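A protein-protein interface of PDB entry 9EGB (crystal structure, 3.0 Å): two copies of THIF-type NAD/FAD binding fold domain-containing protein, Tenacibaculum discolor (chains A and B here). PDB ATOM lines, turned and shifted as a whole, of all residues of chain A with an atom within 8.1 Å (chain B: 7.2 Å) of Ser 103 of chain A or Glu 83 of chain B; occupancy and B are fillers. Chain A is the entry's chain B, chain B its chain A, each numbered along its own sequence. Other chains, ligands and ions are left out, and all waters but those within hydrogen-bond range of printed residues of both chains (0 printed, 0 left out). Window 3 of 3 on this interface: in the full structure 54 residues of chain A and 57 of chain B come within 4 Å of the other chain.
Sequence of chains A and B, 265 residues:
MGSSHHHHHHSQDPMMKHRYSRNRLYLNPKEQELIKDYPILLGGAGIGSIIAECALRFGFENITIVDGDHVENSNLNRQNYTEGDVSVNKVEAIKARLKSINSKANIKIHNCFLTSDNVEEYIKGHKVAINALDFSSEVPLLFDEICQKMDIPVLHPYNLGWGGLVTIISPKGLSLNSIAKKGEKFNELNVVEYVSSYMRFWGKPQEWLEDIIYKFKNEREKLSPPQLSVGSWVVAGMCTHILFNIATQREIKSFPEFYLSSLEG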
ATOM      1  N   LYS A  17      12.892   1.378  19.081  1.00  0.00           N
ATOM      2  CA  LYS A  17      13.818   0.584  19.879  1.00  0.00           C
ATOM      3  C   LYS A  17      14.865  -0.053  18.961  1.00  0.00           C
ATOM      4  O   LYS A  17      14.702  -0.111  17.736  1.00  0.00           O
ATOM      5  CB  LYS A  17      13.090  -0.517  20.673  1.00  0.00           C
ATOM      6  CG  LYS A  17      11.627  -0.243  21.056  1.00  0.00           C
ATOM      7  CD  LYS A  17      11.071  -1.367  21.946  1.00  0.00           C
ATOM      8  CE  LYS A  17       9.689  -1.034  22.511  1.00  0.00           C
ATOM      9  NZ  LYS A  17       9.054  -2.205  23.197  1.00  0.00           N
ATOM     10  N   ARG A  19      15.344  -2.956  18.544  1.00  0.00           N
ATOM     11  CA  ARG A  19      14.623  -4.018  17.845  1.00  0.00           C
ATOM     12  C   ARG A  19      14.079  -3.545  16.496  1.00  0.00           C
ATOM     13  O   ARG A  19      14.076  -4.302  15.516  1.00  0.00           O
ATOM     14  CB  ARG A  19      13.474  -4.470  18.743  1.00  0.00           C
ATOM     15  CG  ARG A  19      12.245  -5.050  18.068  1.00  0.00           C
ATOM     16  CD  ARG A  19      11.085  -5.004  19.068  1.00  0.00           C
ATOM     17  NE  ARG A  19      11.335  -5.779  20.283  1.00  0.00           N
ATOM     18  CZ  ARG A  19      11.130  -7.086  20.395  1.00  0.00           C
ATOM     19  NH1 ARG A  19      10.680  -7.778  19.353  1.00  0.00           N
ATOM     20  NH2 ARG A  19      11.382  -7.697  21.542  1.00  0.00           N
ATOM     21  N   LEU A  56       3.701  -7.907  13.850  1.00  0.00           N
ATOM     22  CA  LEU A  56       4.337  -7.647  15.144  1.00  0.00           C
ATOM     23  C   LEU A  56       5.796  -7.251  14.967  1.00  0.00           C
ATOM     24  O   LEU A  56       6.281  -6.305  15.600  1.00  0.00           O
ATOM     25  CB  LEU A  56       4.226  -8.875  16.054  1.00  0.00           C
ATOM     26  CG  LEU A  56       5.020  -8.785  17.374  1.00  0.00           C
ATOM     27  CD1 LEU A  56       4.549  -7.664  18.273  1.00  0.00           C
ATOM     28  CD2 LEU A  56       5.028 -10.102  18.146  1.00  0.00           C
ATOM     29  N   ARG A  57       6.532  -8.007  14.163  1.00  0.00           N
ATOM     30  CA  ARG A  57       7.933  -7.679  13.962  1.00  0.00           C
ATOM     31  C   ARG A  57       8.081  -6.309  13.319  1.00  0.00           C
ATOM     32  O   ARG A  57       9.009  -5.564  13.649  1.00  0.00           O
ATOM     33  CB  ARG A  57       8.592  -8.757  13.107  1.00  0.00           C
ATOM     34  CG  ARG A  57       8.629 -10.117  13.790  1.00  0.00           C
ATOM     35  CD  ARG A  57       9.453 -11.095  12.996  1.00  0.00           C
ATOM     36  NE  ARG A  57       9.476 -12.418  13.603  1.00  0.00           N
ATOM     37  CZ  ARG A  57      10.277 -12.759  14.608  1.00  0.00           C
ATOM     38  NH1 ARG A  57      11.105 -11.869  15.129  1.00  0.00           N
ATOM     39  NH2 ARG A  57      10.249 -13.991  15.091  1.00  0.00           N
ATOM     40  N   GLU A  61       2.232  -3.523  17.871  1.00  0.00           N
ATOM     41  CA  GLU A  61       2.349  -4.264  19.117  1.00  0.00           C
ATOM     42  C   GLU A  61       1.020  -4.426  19.848  1.00  0.00           C
ATOM     43  O   GLU A  61       1.003  -5.000  20.943  1.00  0.00           O
ATOM     44  CB  GLU A  61       3.361  -3.595  20.055  1.00  0.00           C
ATOM     45  CG  GLU A  61       4.825  -3.665  19.635  1.00  0.00           C
ATOM     46  CD  GLU A  61       5.736  -2.987  20.663  1.00  0.00           C
ATOM     47  OE1 GLU A  61       5.254  -2.693  21.790  1.00  0.00           O
ATOM     48  OE2 GLU A  61       6.915  -2.709  20.333  1.00  0.00           O
ATOM     49  N   LYS A  95      -0.376 -16.636  20.892  1.00  0.00           N
ATOM     50  CA  LYS A  95       0.064 -15.652  21.880  1.00  0.00           C
ATOM     51  C   LYS A  95       1.427 -16.017  22.453  1.00  0.00           C
ATOM     52  O   LYS A  95       2.253 -15.133  22.702  1.00  0.00           O
ATOM     53  CB  LYS A  95      -0.954 -15.472  23.007  1.00  0.00           C
ATOM     54  CG  LYS A  95      -0.475 -14.424  24.017  1.00  0.00           C
ATOM     55  CD  LYS A  95      -1.464 -14.117  25.121  1.00  0.00           C
ATOM     56  CE  LYS A  95      -0.836 -13.173  26.145  1.00  0.00           C
ATOM     57  NZ  LYS A  95      -1.508 -13.158  27.480  1.00  0.00           N
ATOM     58  N   ARG A  97       3.804 -17.747  20.833  1.00  0.00           N
ATOM     59  CA  ARG A  97       4.760 -17.441  19.778  1.00  0.00           C
ATOM     60  C   ARG A  97       5.045 -15.947  19.702  1.00  0.00           C
ATOM     61  O   ARG A  97       6.209 -15.526  19.692  1.00  0.00           O
ATOM     62  CB  ARG A  97       4.223 -17.969  18.447  1.00  0.00           C
ATOM     63  CG  ARG A  97       4.993 -17.523  17.237  1.00  0.00           C
ATOM     64  CD  ARG A  97       6.379 -18.107  17.190  1.00  0.00           C
ATOM     65  NE  ARG A  97       7.057 -17.633  15.996  1.00  0.00           N
ATOM     66  CZ  ARG A  97       8.343 -17.806  15.733  1.00  0.00           C
ATOM     67  NH1 ARG A  97       9.118 -18.461  16.583  1.00  0.00           N
ATOM     68  NH2 ARG A  97       8.847 -17.329  14.606  1.00  0.00           N
ATOM     69  N   LEU A  98       3.990 -15.130  19.652  1.00  0.00           N
ATOM     70  CA  LEU A  98       4.170 -13.687  19.516  1.00  0.00           C
ATOM     71  C   LEU A  98       4.858 -13.086  20.739  1.00  0.00           C
ATOM     72  O   LEU A  98       5.722 -12.214  20.604  1.00  0.00           O
ATOM     73  CB  LEU A  98       2.828 -13.008  19.277  1.00  0.00           C
ATOM     74  CG  LEU A  98       2.157 -13.329  17.951  1.00  0.00           C
ATOM     75  CD1 LEU A  98       0.767 -12.748  18.000  1.00  0.00           C
ATOM     76  CD2 LEU A  98       2.933 -12.804  16.773  1.00  0.00           C
ATOM     77  N   LYS A  99       4.470 -13.512  21.940  1.00  0.00           N
ATOM     78  CA  LYS A  99       5.027 -12.900  23.139  1.00  0.00           C
ATOM     79  C   LYS A  99       6.462 -13.336  23.388  1.00  0.00           C
ATOM     80  O   LYS A  99       7.191 -12.643  24.099  1.00  0.00           O
ATOM     81  CB  LYS A  99       4.140 -13.212  24.343  1.00  0.00           C
ATOM     82  CG  LYS A  99       2.944 -12.259  24.480  1.00  0.00           C
ATOM     83  CD  LYS A  99       3.221 -11.061  25.368  1.00  0.00           C
ATOM     84  CE  LYS A  99       1.939 -10.602  26.054  1.00  0.00           C
ATOM     85  NZ  LYS A  99       2.213  -9.808  27.278  1.00  0.00           N
ATOM     86  N   SER A 100       6.891 -14.456  22.810  1.00  0.00           N
ATOM     87  CA  SER A 100       8.306 -14.812  22.855  1.00  0.00           C
ATOM     88  C   SER A 100       9.138 -13.966  21.890  1.00  0.00           C
ATOM     89  O   SER A 100      10.353 -13.838  22.089  1.00  0.00           O
ATOM     90  CB  SER A 100       8.491 -16.309  22.563  1.00  0.00           C
ATOM     91  OG  SER A 100       8.343 -16.619  21.188  1.00  0.00           O
ATOM     92  N   ILE A 101       8.512 -13.407  20.848  1.00  0.00           N
ATOM     93  CA  ILE A 101       9.158 -12.443  19.961  1.00  0.00           C
ATOM     94  C   ILE A 101       9.259 -11.064  20.610  1.00  0.00           C
ATOM     95  O   ILE A 101      10.286 -10.386  20.500  1.00  0.00           O
ATOM     96  CB  ILE A 101       8.367 -12.356  18.640  1.00  0.00           C
ATOM     97  CG1 ILE A 101       8.416 -13.679  17.874  1.00  0.00           C
ATOM     98  CG2 ILE A 101       8.829 -11.162  17.796  1.00  0.00           C
ATOM     99  CD1 ILE A 101       7.413 -13.750  16.730  1.00  0.00           C
ATOM    100  N   ASN A 102       8.205 -10.624  21.299  1.00  0.00           N
ATOM    101  CA  ASN A 102       8.171  -9.303  21.931  1.00  0.00           C
ATOM    102  C   ASN A 102       7.431  -9.437  23.258  1.00  0.00           C
ATOM    103  O   ASN A 102       6.204  -9.568  23.275  1.00  0.00           O
ATOM    104  CB  ASN A 102       7.505  -8.287  21.005  1.00  0.00           C
ATOM    105  CG  ASN A 102       7.756  -6.833  21.416  1.00  0.00           C
ATOM    106  OD1 ASN A 102       8.011  -6.520  22.585  1.00  0.00           O
ATOM    107  ND2 ASN A 102       7.702  -5.938  20.430  1.00  0.00           N
ATOM    108  N   SER A 103       8.186  -9.452  24.361  1.00  0.00           N
ATOM    109  CA  SER A 103       7.585  -9.621  25.684  1.00  0.00           C
ATOM    110  C   SER A 103       6.721  -8.427  26.095  1.00  0.00           C
ATOM    111  O   SER A 103       5.715  -8.602  26.793  1.00  0.00           O
ATOM    112  CB  SER A 103       8.684  -9.880  26.716  1.00  0.00           C
ATOM    113  OG  SER A 103       9.704  -8.895  26.634  1.00  0.00           O
ATOM    114  N   LYS A 104       7.090  -7.217  25.685  1.00  0.00           N
ATOM    115  CA  LYS A 104       6.316  -6.026  26.016  1.00  0.00           C
ATOM    116  C   LYS A 104       5.141  -5.782  25.065  1.00  0.00           C
ATOM    117  O   LYS A 104       4.505  -4.724  25.155  1.00  0.00           O
ATOM    118  CB  LYS A 104       7.227  -4.786  26.068  1.00  0.00           C
ATOM    119  CG  LYS A 104       8.149  -4.677  27.301  1.00  0.00           C
ATOM    120  CD  LYS A 104       9.353  -5.612  27.308  1.00  0.00           C
ATOM    121  CE  LYS A 104      10.163  -5.432  28.602  1.00  0.00           C
ATOM    122  NZ  LYS A 104      11.439  -6.208  28.629  1.00  0.00           N
ATOM    123  N   ALA A 105       4.841  -6.707  24.154  1.00  0.00           N
ATOM    124  CA  ALA A 105       3.724  -6.514  23.240  1.00  0.00           C
ATOM    125  C   ALA A 105       2.401  -6.733  23.957  1.00  0.00           C
ATOM    126  O   ALA A 105       2.295  -7.527  24.897  1.00  0.00           O
ATOM    127  CB  ALA A 105       3.814  -7.460  22.040  1.00  0.00           C
ATOM    128  N   ASN A 106       1.367  -6.066  23.451  1.00  0.00           N
ATOM    129  CA  ASN A 106       0.039  -6.099  24.054  1.00  0.00           C
ATOM    130  C   ASN A 106      -0.831  -7.046  23.228  1.00  0.00           C
ATOM    131  O   ASN A 106      -1.546  -6.649  22.310  1.00  0.00           O
ATOM    132  CB  ASN A 106      -0.518  -4.682  24.113  1.00  0.00           C
ATOM    133  CG  ASN A 106      -1.699  -4.555  25.032  1.00  0.00           C
ATOM    134  OD1 ASN A 106      -2.503  -5.475  25.167  1.00  0.00           O
ATOM    135  ND2 ASN A 106      -1.811  -3.405  25.680  1.00  0.00           N
ATOM    136  N   ILE A 107      -0.731  -8.332  23.548  1.00  0.00           N
ATOM    137  CA  ILE A 107      -1.408  -9.389  22.804  1.00  0.00           C
ATOM    138  C   ILE A 107      -2.553  -9.947  23.638  1.00  0.00           C
ATOM    139  O   ILE A 107      -2.322 -10.669  24.619  1.00  0.00           O
ATOM    140  CB  ILE A 107      -0.438 -10.499  22.387  1.00  0.00           C
ATOM    141  CG1 ILE A 107       0.788  -9.898  21.678  1.00  0.00           C
ATOM    142  CG2 ILE A 107      -1.168 -11.541  21.544  1.00  0.00           C
ATOM    143  CD1 ILE A 107       0.474  -9.138  20.400  1.00  0.00           C
ATOM    144  N   VAL B  71      22.554 -14.236  16.971  1.00  0.00           N
ATOM    145  CA  VAL B  71      21.276 -13.537  16.934  1.00  0.00           C
ATOM    146  C   VAL B  71      21.428 -12.223  17.690  1.00  0.00           C
ATOM    147  O   VAL B  71      21.839 -12.198  18.859  1.00  0.00           O
ATOM    148  CB  VAL B  71      20.160 -14.406  17.536  1.00  0.00           C
ATOM    149  CG1 VAL B  71      18.852 -13.611  17.643  1.00  0.00           C
ATOM    150  CG2 VAL B  71      19.974 -15.677  16.725  1.00  0.00           C
ATOM    151  N   ASN B  73      19.643  -8.212  18.624  1.00  0.00           N
ATOM    152  CA  ASN B  73      18.352  -7.589  18.874  1.00  0.00           C
ATOM    153  C   ASN B  73      17.744  -7.061  17.580  1.00  0.00           C
ATOM    154  O   ASN B  73      16.551  -7.251  17.322  1.00  0.00           O
ATOM    155  CB  ASN B  73      18.495  -6.477  19.901  1.00  0.00           C
ATOM    156  CG  ASN B  73      17.986  -6.892  21.243  1.00  0.00           C
ATOM    157  OD1 ASN B  73      16.791  -6.795  21.520  1.00  0.00           O
ATOM    158  ND2 ASN B  73      18.883  -7.384  22.090  1.00  0.00           N
ATOM    159  N   LEU B  76      15.153  -8.886  15.064  1.00  0.00           N
ATOM    160  CA  LEU B  76      13.799  -9.301  15.371  1.00  0.00           C
ATOM    161  C   LEU B  76      12.761  -8.611  14.493  1.00  0.00           C
ATOM    162  O   LEU B  76      11.624  -9.083  14.416  1.00  0.00           O
ATOM    163  CB  LEU B  76      13.537  -9.041  16.851  1.00  0.00           C
ATOM    164  CG  LEU B  76      14.518  -9.813  17.737  1.00  0.00           C
ATOM    165  CD1 LEU B  76      14.315  -9.516  19.222  1.00  0.00           C
ATOM    166  CD2 LEU B  76      14.445 -11.298  17.460  1.00  0.00           C
ATOM    167  N   TYR B  81      13.701 -15.165  14.690  1.00  0.00           N
ATOM    168  CA  TYR B  81      14.281 -15.423  16.007  1.00  0.00           C
ATOM    169  C   TYR B  81      13.453 -14.728  17.083  1.00  0.00           C
ATOM    170  O   TYR B  81      12.650 -13.827  16.807  1.00  0.00           O
ATOM    171  CB  TYR B  81      15.766 -14.999  16.095  1.00  0.00           C
ATOM    172  CG  TYR B  81      16.610 -15.620  15.003  1.00  0.00           C
ATOM    173  CD1 TYR B  81      16.932 -16.972  15.019  1.00  0.00           C
ATOM    174  CD2 TYR B  81      17.076 -14.847  13.939  1.00  0.00           C
ATOM    175  CE1 TYR B  81      17.691 -17.542  13.990  1.00  0.00           C
ATOM    176  CE2 TYR B  81      17.830 -15.398  12.916  1.00  0.00           C
ATOM    177  CZ  TYR B  81      18.134 -16.745  12.943  1.00  0.00           C
ATOM    178  OH  TYR B  81      18.887 -17.282  11.923  1.00  0.00           O
ATOM    179  N   THR B  82      13.662 -15.165  18.320  1.00  0.00           N
ATOM    180  CA  THR B  82      12.918 -14.698  19.478  1.00  0.00           C
ATOM    181  C   THR B  82      13.843 -14.009  20.478  1.00  0.00           C
ATOM    182  O   THR B  82      15.069 -14.037  20.347  1.00  0.00           O
ATOM    183  CB  THR B  82      12.185 -15.870  20.138  1.00  0.00           C
ATOM    184  OG1 THR B  82      13.146 -16.808  20.634  1.00  0.00           O
ATOM    185  CG2 THR B  82      11.312 -16.577  19.123  1.00  0.00           C
ATOM    186  N   GLU B  83      13.234 -13.361  21.482  1.00  0.00           N
ATOM    187  CA  GLU B  83      14.026 -12.719  22.528  1.00  0.00           C
ATOM    188  C   GLU B  83      14.940 -13.722  23.223  1.00  0.00           C
ATOM    189  O   GLU B  83      16.053 -13.372  23.634  1.00  0.00           O
ATOM    190  CB  GLU B  83      13.113 -12.043  23.546  1.00  0.00           C
ATOM    191  CG  GLU B  83      12.353 -10.839  23.015  1.00  0.00           C
ATOM    192  CD  GLU B  83      11.576 -10.102  24.102  1.00  0.00           C
ATOM    193  OE1 GLU B  83      11.029  -9.015  23.812  1.00  0.00           O
ATOM    194  OE2 GLU B  83      11.511 -10.616  25.244  1.00  0.00           O
ATOM    195  N   GLY B  84      14.489 -14.969  23.368  1.00  0.00           N
ATOM    196  CA  GLY B  84      15.315 -15.990  23.988  1.00  0.00           C
ATOM    197  C   GLY B  84      16.498 -16.414  23.144  1.00  0.00           C
ATOM    198  O   GLY B  84      17.468 -16.968  23.680  1.00  0.00           O
ATOM    199  N   ASP B  85      16.433 -16.171  21.835  1.00  0.00           N
ATOM    200  CA  ASP B  85      17.503 -16.534  20.916  1.00  0.00           C
ATOM    201  C   ASP B  85      18.686 -15.565  20.953  1.00  0.00           C
ATOM    202  O   ASP B  85      19.753 -15.900  20.437  1.00  0.00           O
ATOM    203  CB  ASP B  85      16.946 -16.619  19.491  1.00  0.00           C
ATOM    204  CG  ASP B  85      15.959 -17.768  19.313  1.00  0.00           C
ATOM    205  OD1 ASP B  85      16.129 -18.810  19.998  1.00  0.00           O
ATOM    206  OD2 ASP B  85      15.005 -17.618  18.498  1.00  0.00           O
ATOM    207  N   VAL B  86      18.521 -14.370  21.519  1.00  0.00           N
ATOM    208  CA  VAL B  86      19.561 -13.350  21.430  1.00  0.00           C
ATOM    209  C   VAL B  86      20.827 -13.827  22.125  1.00  0.00           C
ATOM    210  O   VAL B  86      20.783 -14.326  23.256  1.00  0.00           O
ATOM    211  CB  VAL B  86      19.056 -12.026  22.016  1.00  0.00           C
ATOM    212  CG1 VAL B  86      20.181 -11.020  22.127  1.00  0.00           C
ATOM    213  CG2 VAL B  86      17.975 -11.478  21.141  1.00  0.00           C
ATOM    214  N   SER B  87      21.965 -13.668  21.443  1.00  0.00           N
ATOM    215  CA  SER B  87      23.329 -14.084  21.807  1.00  0.00           C
ATOM    216  C   SER B  87      23.631 -15.530  21.425  1.00  0.00           C
ATOM    217  O   SER B  87      24.767 -15.963  21.605  1.00  0.00           O
ATOM    218  CB  SER B  87      23.629 -13.914  23.306  1.00  0.00           C
ATOM    219  OG  SER B  87      23.459 -12.566  23.701  1.00  0.00           O
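The backbone NH (N) of Thr 82 of chain B sits at hydrogen-bond distance from the side-chain carboxylate (OD2) of Asp 85 of chain B, at 2.8 Å.
The guanidinium group of Arg 19 of chain A sits at hydrogen-bond distance from the backbone carbonyl oxygen of Ile 101 of chain A.
The side-chain carboxylate (OE2) of Glu 61 of chain A sits at hydrogen-bond distance from the side-chain amide nitrogen (ND2) of Asn 102 of chain A, at 3.3 Å.
O of Arg 97 of chain A lies within hydrogen-bond range of OG of Ser 100 of chain A (2.8 Å).
OD1 of Asn 102 of chain A sits close to N of Lys 104 of chain A, 3.3 Å away.
Of the printed residues of chain B, Arg 57 of chain A touches Leu 76 and Tyr 81.
Leu 98 of chain A touches none of the printed residues of chain B.
Of chain B, only Glu 83 (2.9 Å) comes within 4 Å of Ser 103 of chain A.
Printed residues of chain A within 4 Å of Leu 76 of chain B: Arg 57 (2.9 Å).
Of the printed residues of chain A, Tyr 81 of chain B touches Arg 57 (3.0 Å).
Glu 83 of chain B touches just these residues of chain A: Arg 19, Ser 100, Ile 101, Asn 102 and Ser 103.
No residue of chain A comes within 4 Å of Gly 84 of chain B.
The nearest printed residue of chain B that does not touch Ser 103 of chain A is Leu 76 of chain B (8.0 Å).
The nearest printed residue of chain B that does not touch Ser 100 of chain A is Gly 84 of chain B (4.5 Å).
Among the printed residues, pairs that only touch across the chains: Ile 101 of chain A with Glu 83 of chain B (3.3 Å), Ser 100 of chain A with Thr 82 of chain B (3.4 Å), Asn 102 of chain A with Glu 83 of chain B (3.4 Å), Arg 19 of chain A with Asn 73 of chain B (3.8 Å) and Arg 97 of chain A with Thr 82 of chain B (3.8 Å).
Printed residues of chain B that touch a printed residue of chain A: Asn 73, Leu 76, Tyr 81, Thr 82 and Glu 83.
Printed residues of chain A that touch a printed residue of chain B: Arg 19, Arg 57, Arg 97, Ser 100, Ile 101, Asn 102 and Ser 103.
Among the printed residues, Asp or Glu carboxylates within 4 Å of a Lys or Arg side-chain nitrogen of the other chain: Arg 19 of chain A with Glu 83 of chain B (2.6 Å).
The backbone carbonyl oxygen (O) of Leu 76 of chain B lies within hydrogen-bond range of the guanidinium group (NH1) of Arg 57 of chain A (2.9 Å).
O of Tyr 81 of chain B is in hydrogen-bond range of NH2 of Arg 57 of chain A, 3.0 Å away.
OE1 of Glu 83 of chain B is in salt-bridge range of NH2 of Arg 19 of chain A, at 2.6 Å.
The backbone carbonyl oxygen (O) of Ser 100 of chain A lies within hydrogen-bond range of the backbone NH (N) of Glu 83 of chain B (3.0 Å).
The side-chain carboxylate (OE2) of Glu 83 of chain B is in hydrogen-bond range of the side-chain hydroxyl (OG) of Ser 103 of chain A.
No position is printed for both chains.
Of the 10 pairs that touch across the chains among the printed residues, none has its exchanged pair printed and touching as well.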
